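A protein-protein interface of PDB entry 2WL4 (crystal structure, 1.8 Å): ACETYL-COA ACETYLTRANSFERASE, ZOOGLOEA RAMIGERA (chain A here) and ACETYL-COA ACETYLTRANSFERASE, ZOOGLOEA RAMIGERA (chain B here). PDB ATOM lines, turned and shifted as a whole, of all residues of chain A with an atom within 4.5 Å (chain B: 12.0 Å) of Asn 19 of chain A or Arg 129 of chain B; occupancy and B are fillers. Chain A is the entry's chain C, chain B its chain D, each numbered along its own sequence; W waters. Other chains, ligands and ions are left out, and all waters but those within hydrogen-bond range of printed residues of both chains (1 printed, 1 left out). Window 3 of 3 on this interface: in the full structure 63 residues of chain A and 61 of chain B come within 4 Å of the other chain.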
ATOM      1  N   SER A  17      32.697  13.128 -20.844  1.00  0.00           N
ATOM      2  CA  SER A  17      32.742  12.283 -19.657  1.00  0.00           C
ATOM      3  C   SER A  17      31.365  12.197 -19.013  1.00  0.00           C
ATOM      4  O   SER A  17      30.488  13.016 -19.290  1.00  0.00           O
ATOM      5  CB  SER A  17      33.763  12.820 -18.653  1.00  0.00           C
ATOM      6  OG  SER A  17      35.027  13.022 -19.266  1.00  0.00           O
ATOM      7  N   PHE A  18      31.182  11.206 -18.148  1.00  0.00           N
ATOM      8  CA  PHE A  18      29.896  10.999 -17.496  1.00  0.00           C
ATOM      9  C   PHE A  18      29.448  12.277 -16.803  1.00  0.00           C
ATOM     10  O   PHE A  18      30.168  12.830 -15.971  1.00  0.00           O
ATOM     11  CB  PHE A  18      29.977   9.844 -16.498  1.00  0.00           C
ATOM     12  CG  PHE A  18      28.648   9.205 -16.196  1.00  0.00           C
ATOM     13  CD1 PHE A  18      27.797   8.828 -17.224  1.00  0.00           C
ATOM     14  CD2 PHE A  18      28.255   8.968 -14.885  1.00  0.00           C
ATOM     15  CE1 PHE A  18      26.573   8.237 -16.952  1.00  0.00           C
ATOM     16  CE2 PHE A  18      27.034   8.374 -14.607  1.00  0.00           C
ATOM     17  CZ  PHE A  18      26.195   8.006 -15.641  1.00  0.00           C
ATOM     18  N   ASN A  19      28.262  12.750 -17.170  1.00  0.00           N
ATOM     19  CA  ASN A  19      27.682  13.940 -16.564  1.00  0.00           C
ATOM     20  C   ASN A  19      28.599  15.163 -16.660  1.00  0.00           C
ATOM     21  O   ASN A  19      28.646  16.001 -15.758  1.00  0.00           O
ATOM     22  CB  ASN A  19      27.276  13.638 -15.123  1.00  0.00           C
ATOM     23  CG  ASN A  19      26.227  12.544 -15.042  1.00  0.00           C
ATOM     24  OD1 ASN A  19      25.302  12.501 -15.855  1.00  0.00           O
ATOM     25  ND2 ASN A  19      26.374  11.642 -14.074  1.00  0.00           N
ATOM     26  N   GLY A  20      29.317  15.255 -17.776  1.00  0.00           N
ATOM     27  CA  GLY A  20      30.224  16.359 -18.024  1.00  0.00           C
ATOM     28  C   GLY A  20      29.719  17.340 -19.071  1.00  0.00           C
ATOM     29  O   GLY A  20      28.649  17.926 -18.921  1.00  0.00           O
ATOM     30  N   ALA A  23      26.301  16.521 -20.361  1.00  0.00           N
ATOM     31  CA  ALA A  23      25.474  15.934 -19.316  1.00  0.00           C
ATOM     32  C   ALA A  23      23.974  16.169 -19.533  1.00  0.00           C
ATOM     33  O   ALA A  23      23.151  15.375 -19.089  1.00  0.00           O
ATOM     34  CB  ALA A  23      25.899  16.454 -17.959  1.00  0.00           C
ATOM     35  N   MET A 119      24.743   8.453 -22.354  1.00  0.00           N
ATOM     36  CA  MET A 119      24.586   7.659 -21.146  1.00  0.00           C
ATOM     37  C   MET A 119      24.255   8.605 -20.000  1.00  0.00           C
ATOM     38  O   MET A 119      23.501   8.268 -19.079  1.00  0.00           O
ATOM     39  CB  MET A 119      25.862   6.857 -20.870  1.00  0.00           C
ATOM     40  CG  MET A 119      26.233   5.924 -22.013  1.00  0.00           C
ATOM     41  SD  MET A 119      27.820   5.083 -21.832  1.00  0.00           S
ATOM     42  CE  MET A 119      27.426   3.949 -20.499  1.00  0.00           C
ATOM     43  N   SER A 120      24.801   9.811 -20.086  1.00  0.00           N
ATOM     44  CA  SER A 120      24.487  10.861 -19.131  1.00  0.00           C
ATOM     45  C   SER A 120      22.977  11.103 -19.018  1.00  0.00           C
ATOM     46  O   SER A 120      22.464  11.334 -17.922  1.00  0.00           O
ATOM     47  CB  SER A 120      25.216  12.159 -19.509  1.00  0.00           C
ATOM     48  OG  SER A 120      26.616  12.027 -19.336  1.00  0.00           O
ATOM     49  N   ALA A 122      20.489   8.960 -19.811  1.00  0.00           N
ATOM     50  CA  ALA A 122      19.697   7.746 -19.565  1.00  0.00           C
ATOM     51  C   ALA A 122      18.940   7.792 -18.234  1.00  0.00           C
ATOM     52  O   ALA A 122      19.564   7.878 -17.176  1.00  0.00           O
ATOM     53  CB  ALA A 122      20.593   6.525 -19.613  1.00  0.00           C
ATOM     54  N   HIS A 124      16.184   6.709 -15.026  1.00  0.00           N
ATOM     55  CA  HIS A 124      15.807   5.562 -14.223  1.00  0.00           C
ATOM     56  C   HIS A 124      14.332   5.306 -14.471  1.00  0.00           C
ATOM     57  O   HIS A 124      13.570   6.243 -14.717  1.00  0.00           O
ATOM     58  CB  HIS A 124      16.035   5.848 -12.741  1.00  0.00           C
ATOM     59  CG  HIS A 124      17.479   5.929 -12.357  1.00  0.00           C
ATOM     60  ND1 HIS A 124      18.316   6.925 -12.818  1.00  0.00           N
ATOM     61  CD2 HIS A 124      18.236   5.151 -11.549  1.00  0.00           C
ATOM     62  CE1 HIS A 124      19.522   6.752 -12.312  1.00  0.00           C
ATOM     63  NE2 HIS A 124      19.501   5.680 -11.536  1.00  0.00           N
ATOM     64  N   ASP A 141      18.219   1.971 -12.838  1.00  0.00           N
ATOM     65  CA  ASP A 141      19.094   2.744 -13.701  1.00  0.00           C
ATOM     66  C   ASP A 141      19.174   2.065 -15.057  1.00  0.00           C
ATOM     67  O   ASP A 141      19.893   1.079 -15.223  1.00  0.00           O
ATOM     68  CB  ASP A 141      20.484   2.838 -13.076  1.00  0.00           C
ATOM     69  CG  ASP A 141      21.342   3.885 -13.728  1.00  0.00           C
ATOM     70  OD1 ASP A 141      21.315   3.985 -14.980  1.00  0.00           O
ATOM     71  OD2 ASP A 141      22.047   4.605 -12.987  1.00  0.00           O
ATOM     72  N   MET A 143      20.670   2.824 -17.765  1.00  0.00           N
ATOM     73  CA  MET A 143      22.052   2.737 -18.238  1.00  0.00           C
ATOM     74  C   MET A 143      22.702   1.429 -17.786  1.00  0.00           C
ATOM     75  O   MET A 143      23.335   0.731 -18.580  1.00  0.00           O
ATOM     76  CB  MET A 143      22.882   3.923 -17.741  1.00  0.00           C
ATOM     77  CG  MET A 143      24.350   3.874 -18.172  1.00  0.00           C
ATOM     78  SD  MET A 143      25.417   5.050 -17.297  1.00  0.00           S
ATOM     79  CE  MET A 143      25.524   4.255 -15.691  1.00  0.00           C
ATOM     80  N   ASP A 251      29.337  10.089 -23.264  1.00  0.00           N
ATOM     81  CA  ASP A 251      28.365  10.583 -24.240  1.00  0.00           C
ATOM     82  C   ASP A 251      29.084  11.052 -25.496  1.00  0.00           C
ATOM     83  O   ASP A 251      30.151  11.659 -25.420  1.00  0.00           O
ATOM     84  CB  ASP A 251      27.570  11.771 -23.694  1.00  0.00           C
ATOM     85  CG  ASP A 251      27.362  11.700 -22.205  1.00  0.00           C
ATOM     86  OD1 ASP A 251      26.991  10.618 -21.698  1.00  0.00           O
ATOM     87  OD2 ASP A 251      27.560  12.743 -21.548  1.00  0.00           O
ATOM     88  N   ALA B  60      12.771  -0.436 -22.506  1.00  0.00           N
ATOM     89  CA  ALA B  60      13.311   0.093 -21.254  1.00  0.00           C
ATOM     90  C   ALA B  60      13.122  -0.868 -20.079  1.00  0.00           C
ATOM     91  O   ALA B  60      12.007  -1.318 -19.806  1.00  0.00           O
ATOM     92  CB  ALA B  60      12.697   1.451 -20.927  1.00  0.00           C
ATOM     93  N   GLY B  61      14.224  -1.170 -19.395  1.00  0.00           N
ATOM     94  CA  GLY B  61      14.204  -1.955 -18.173  1.00  0.00           C
ATOM     95  C   GLY B  61      14.200  -3.461 -18.341  1.00  0.00           C
ATOM     96  O   GLY B  61      14.214  -4.199 -17.354  1.00  0.00           O
ATOM     97  N   HIS B 124       7.548   3.688 -16.405  1.00  0.00           N
ATOM     98  CA  HIS B 124       7.662   5.145 -16.290  1.00  0.00           C
ATOM     99  C   HIS B 124       9.090   5.510 -15.922  1.00  0.00           C
ATOM    100  O   HIS B 124       9.799   4.708 -15.308  1.00  0.00           O
ATOM    101  CB  HIS B 124       6.725   5.676 -15.214  1.00  0.00           C
ATOM    102  CG  HIS B 124       5.289   5.746 -15.638  1.00  0.00           C
ATOM    103  ND1 HIS B 124       4.537   4.626 -15.930  1.00  0.00           N
ATOM    104  CD2 HIS B 124       4.462   6.805 -15.805  1.00  0.00           C
ATOM    105  CE1 HIS B 124       3.310   4.994 -16.255  1.00  0.00           C
ATOM    106  NE2 HIS B 124       3.236   6.312 -16.181  1.00  0.00           N
ATOM    107  N   CYS B 125       9.522   6.718 -16.274  1.00  0.00           N
ATOM    108  CA  CYS B 125      10.912   7.076 -16.051  1.00  0.00           C
ATOM    109  C   CYS B 125      11.139   8.572 -15.950  1.00  0.00           C
ATOM    110  O   CYS B 125      10.257   9.385 -16.257  1.00  0.00           O
ATOM    111  CB  CYS B 125      11.781   6.533 -17.187  1.00  0.00           C
ATOM    112  SG  CYS B 125      11.739   7.556 -18.693  1.00  0.00           S
ATOM    113  N   ALA B 126      12.350   8.917 -15.535  1.00  0.00           N
ATOM    114  CA  ALA B 126      12.786  10.292 -15.481  1.00  0.00           C
ATOM    115  C   ALA B 126      14.295  10.345 -15.409  1.00  0.00           C
ATOM    116  O   ALA B 126      14.935   9.423 -14.899  1.00  0.00           O
ATOM    117  CB  ALA B 126      12.195  10.987 -14.267  1.00  0.00           C
ATOM    118  N   HIS B 127      14.864  11.438 -15.901  1.00  0.00           N
ATOM    119  CA  HIS B 127      16.289  11.644 -15.757  1.00  0.00           C
ATOM    120  C   HIS B 127      16.572  12.320 -14.420  1.00  0.00           C
ATOM    121  O   HIS B 127      16.181  13.462 -14.204  1.00  0.00           O
ATOM    122  CB  HIS B 127      16.849  12.464 -16.918  1.00  0.00           C
ATOM    123  CG  HIS B 127      18.323  12.700 -16.820  1.00  0.00           C
ATOM    124  ND1 HIS B 127      18.868  13.954 -16.669  1.00  0.00           N
ATOM    125  CD2 HIS B 127      19.364  11.832 -16.819  1.00  0.00           C
ATOM    126  CE1 HIS B 127      20.185  13.853 -16.595  1.00  0.00           C
ATOM    127  NE2 HIS B 127      20.509  12.577 -16.681  1.00  0.00           N
ATOM    128  N   LEU B 128      17.273  11.605 -13.541  1.00  0.00           N
ATOM    129  CA  LEU B 128      17.498  12.045 -12.166  1.00  0.00           C
ATOM    130  C   LEU B 128      18.975  12.041 -11.825  1.00  0.00           C
ATOM    131  O   LEU B 128      19.371  12.319 -10.690  1.00  0.00           O
ATOM    132  CB  LEU B 128      16.742  11.117 -11.207  1.00  0.00           C
ATOM    133  CG  LEU B 128      15.311  10.790 -11.642  1.00  0.00           C
ATOM    134  CD1 LEU B 128      14.710   9.696 -10.762  1.00  0.00           C
ATOM    135  CD2 LEU B 128      14.440  12.047 -11.639  1.00  0.00           C
ATOM    136  N   ARG B 129      19.797  11.734 -12.820  1.00  0.00           N
ATOM    137  CA  ARG B 129      21.234  11.650 -12.617  1.00  0.00           C
ATOM    138  C   ARG B 129      21.791  13.002 -12.193  1.00  0.00           C
ATOM    139  O   ARG B 129      22.653  13.085 -11.316  1.00  0.00           O
ATOM    140  CB  ARG B 129      21.914  11.172 -13.899  1.00  0.00           C
ATOM    141  CG  ARG B 129      23.091  10.258 -13.661  1.00  0.00           C
ATOM    142  CD  ARG B 129      23.619   9.691 -14.973  1.00  0.00           C
ATOM    143  NE  ARG B 129      22.675   8.797 -15.637  1.00  0.00           N
ATOM    144  CZ  ARG B 129      22.403   7.556 -15.241  1.00  0.00           C
ATOM    145  NH1 ARG B 129      22.981   7.056 -14.153  1.00  0.00           N
ATOM    146  NH2 ARG B 129      21.529   6.819 -15.921  1.00  0.00           N
ATOM    147  N   GLY B 130      21.296  14.061 -12.825  1.00  0.00           N
ATOM    148  CA  GLY B 130      21.678  15.412 -12.459  1.00  0.00           C
ATOM    149  C   GLY B 130      20.930  15.887 -11.230  1.00  0.00           C
ATOM    150  O   GLY B 130      21.405  16.745 -10.494  1.00  0.00           O
ATOM    151  N   GLY B 131      19.749  15.320 -11.008  1.00  0.00           N
ATOM    152  CA  GLY B 131      18.945  15.673  -9.854  1.00  0.00           C
ATOM    153  C   GLY B 131      17.777  16.578 -10.188  1.00  0.00           C
ATOM    154  O   GLY B 131      17.615  17.023 -11.327  1.00  0.00           O
ATOM    155  N   VAL B 132      16.954  16.843  -9.181  1.00  0.00           N
ATOM    156  CA  VAL B 132      15.803  17.721  -9.317  1.00  0.00           C
ATOM    157  C   VAL B 132      15.837  18.671  -8.128  1.00  0.00           C
ATOM    158  O   VAL B 132      15.172  18.445  -7.118  1.00  0.00           O
ATOM    159  CB  VAL B 132      14.498  16.909  -9.315  1.00  0.00           C
ATOM    160  CG1 VAL B 132      13.292  17.810  -9.552  1.00  0.00           C
ATOM    161  CG2 VAL B 132      14.565  15.814 -10.370  1.00  0.00           C
ATOM    162  N   LYS B 133      16.626  19.731  -8.261  1.00  0.00           N
ATOM    163  CA  LYS B 133      16.975  20.602  -7.141  1.00  0.00           C
ATOM    164  C   LYS B 133      15.796  21.049  -6.270  1.00  0.00           C
ATOM    165  O   LYS B 133      15.913  21.090  -5.053  1.00  0.00           O
ATOM    166  CB  LYS B 133      17.758  21.815  -7.640  1.00  0.00           C
ATOM    167  CG  LYS B 133      19.091  21.459  -8.280  1.00  0.00           C
ATOM    168  CD  LYS B 133      19.976  20.694  -7.312  1.00  0.00           C
ATOM    169  CE  LYS B 133      21.270  20.262  -7.977  1.00  0.00           C
ATOM    170  NZ  LYS B 133      21.008  19.444  -9.188  1.00  0.00           N
ATOM    171  N   PHE B 137       8.025  17.526 -10.568  1.00  0.00           N
ATOM    172  CA  PHE B 137       8.464  17.067 -11.892  1.00  0.00           C
ATOM    173  C   PHE B 137       7.599  15.912 -12.399  1.00  0.00           C
ATOM    174  O   PHE B 137       6.673  15.477 -11.704  1.00  0.00           O
ATOM    175  CB  PHE B 137       9.943  16.669 -11.883  1.00  0.00           C
ATOM    176  CG  PHE B 137      10.225  15.342 -11.232  1.00  0.00           C
ATOM    177  CD1 PHE B 137      10.262  14.176 -11.986  1.00  0.00           C
ATOM    178  CD2 PHE B 137      10.466  15.260  -9.874  1.00  0.00           C
ATOM    179  CE1 PHE B 137      10.529  12.956 -11.394  1.00  0.00           C
ATOM    180  CE2 PHE B 137      10.736  14.047  -9.274  1.00  0.00           C
ATOM    181  CZ  PHE B 137      10.764  12.890 -10.035  1.00  0.00           C
ATOM    182  N   LYS B 138       7.903  15.426 -13.607  1.00  0.00           N
ATOM    183  CA  LYS B 138       7.151  14.322 -14.213  1.00  0.00           C
ATOM    184  C   LYS B 138       7.934  13.020 -14.331  1.00  0.00           C
ATOM    185  O   LYS B 138       9.105  13.003 -14.716  1.00  0.00           O
ATOM    186  CB  LYS B 138       6.651  14.705 -15.609  1.00  0.00           C
ATOM    187  CG  LYS B 138       5.696  15.889 -15.661  1.00  0.00           C
ATOM    188  CD  LYS B 138       5.574  16.399 -17.091  1.00  0.00           C
ATOM    189  CE  LYS B 138       4.833  17.723 -17.158  1.00  0.00           C
ATOM    190  NZ  LYS B 138       4.734  18.222 -18.560  1.00  0.00           N
ATOM    191  N   MET B 139       7.264  11.922 -14.005  1.00  0.00           N
ATOM    192  CA  MET B 139       7.686  10.595 -14.444  1.00  0.00           C
ATOM    193  C   MET B 139       6.904  10.340 -15.759  1.00  0.00           C
ATOM    194  O   MET B 139       5.664  10.432 -15.781  1.00  0.00           O
ATOM    195  CB  MET B 139       7.369   9.555 -13.337  1.00  0.00           C
ATOM    196  CG  MET B 139       8.229   9.644 -12.131  1.00  0.00           C
ATOM    197  SD  MET B 139       9.855   8.871 -12.363  1.00  0.00           S
ATOM    198  CE  MET B 139       9.408   7.138 -12.444  1.00  0.00           C
HETATM  199  O   HOH W   1      18.707   9.183 -14.655  1.00  0.00           O
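OD2 of Asp 141 of chain A is in hydrogen-bond range of NE2 of His 124 of chain A (3.1 Å).
OD2 of Asp 251 of chain A lies within hydrogen-bond range of OG of Ser 120 of chain A (2.5 Å).
The side-chain carboxylate of Asp 251 of chain A sits at hydrogen-bond distance from the backbone NH of Met 119 of chain A (3.2 Å).
OD1 of Asp 141 of chain A is in hydrogen-bond range of N of Met 143 of chain A, at 3.1 Å.
The backbone NH of Asn 19 of chain A lies within hydrogen-bond range of the side-chain hydroxyl of Ser 120 of chain A (2.8 Å).
Of the 12 printed residues of chain A, 8 touch a printed residue of chain B.
Hydrophobic or aromatic side chains of chain A that line the printed part of chain B: Phe 18, Ala 122, His 124 and Met 143.
Among the printed residues, 12 pairs touch across the chains.
Among the printed residues, Asp or Glu carboxylates within 4 Å of a Lys or Arg side-chain nitrogen of the other chain: Asp 141 of chain A with Arg 129 of chain B.
Among the printed residues, merely in contact across the chains: His 124 of chain A with Cys 125 of chain B (3.1 Å), Phe 18 of chain A with Arg 129 of chain B (3.1 Å), Asn 19 of chain A with Arg 129 of chain B (3.4 Å), Met 119 of chain A with Arg 129 of chain B (3.6 Å), Met 143 of chain A with Arg 129 of chain B (3.7 Å), His 124 of chain A with Arg 129 of chain B (3.9 Å) and Ala 122 of chain A with His 127 of chain B (3.98 Å).
O of Ser 120 of chain A is in hydrogen-bond range of NE2 of His 127 of chain B, 2.6 Å away.
The backbone NH of His 124 of chain A lies within hydrogen-bond range of the backbone carbonyl oxygen of Ala 126 of chain B (3.0 Å).
The backbone carbonyl oxygen (O) of Ala 122 of chain A sits at hydrogen-bond distance from the guanidinium group (NH2) of Arg 129 of chain B (2.6 Å).
NE of Arg 129 of chain B sits at hydrogen-bond distance from O of Ser 120 of chain A (3.4 Å).
NH1 of Arg 129 of chain B is in salt-bridge range of OD2 of Asp 141 of chain A (2.9 Å).
Water W1 lies within hydrogen-bond range of ND1 of His 124 of chain A (2.9 Å), O of Ala 122 of chain A (3.0 Å), N of Leu 128 of chain B (3.0 Å) and N of Arg 129 of chain B (3.3 Å).
Asn 19 of chain A touches just one residue of chain B: Arg 129 (3.4 Å).
Of chain A, only Phe 18 (3.1 Å), Asn 19 (3.4 Å), Met 119 (3.6 Å), Ser 120 (3.4 Å), Ala 122 (2.6 Å), His 124 (3.9 Å), Asp 141 (2.9 Å) and Met 143 (3.7 Å) come within 4 Å of Arg 129 of chain B.
No residue of chain B comes within 4 Å of Ser 17 of chain A.
Of chain B, only Arg 129 (3.1 Å) comes within 4 Å of Phe 18 of chain A.
No residue of chain B comes within 4 Å of Ala 23 of chain A.
Ser 120 of chain A touches just these residues of chain B: His 127 and Arg 129.
Ala 122 of chain A touches just these residues of chain B: His 127 (3.98 Å) and Arg 129 (2.6 Å).
Of chain B, only Arg 129 comes within 4 Å of Met 143 of chain A.
Of the printed residues of chain B, Met 119 of chain A touches Arg 129 (3.6 Å).
Of the printed residues of chain A, Ala 126 of chain B touches His 124 (3.0 Å).
Lys 138 of chain B touches none of the printed residues of chain A.
The nearest residue of chain B that does not touch Asn 19 of chain A is His 127 of chain B (4.9 Å).
The nearest printed residue of chain A that does not touch Arg 129 of chain B is Ala 23 of chain A (6.8 Å).
The nearest printed residue of chain B that does not touch His 124 of chain A is His 124 of chain B (4.1 Å).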
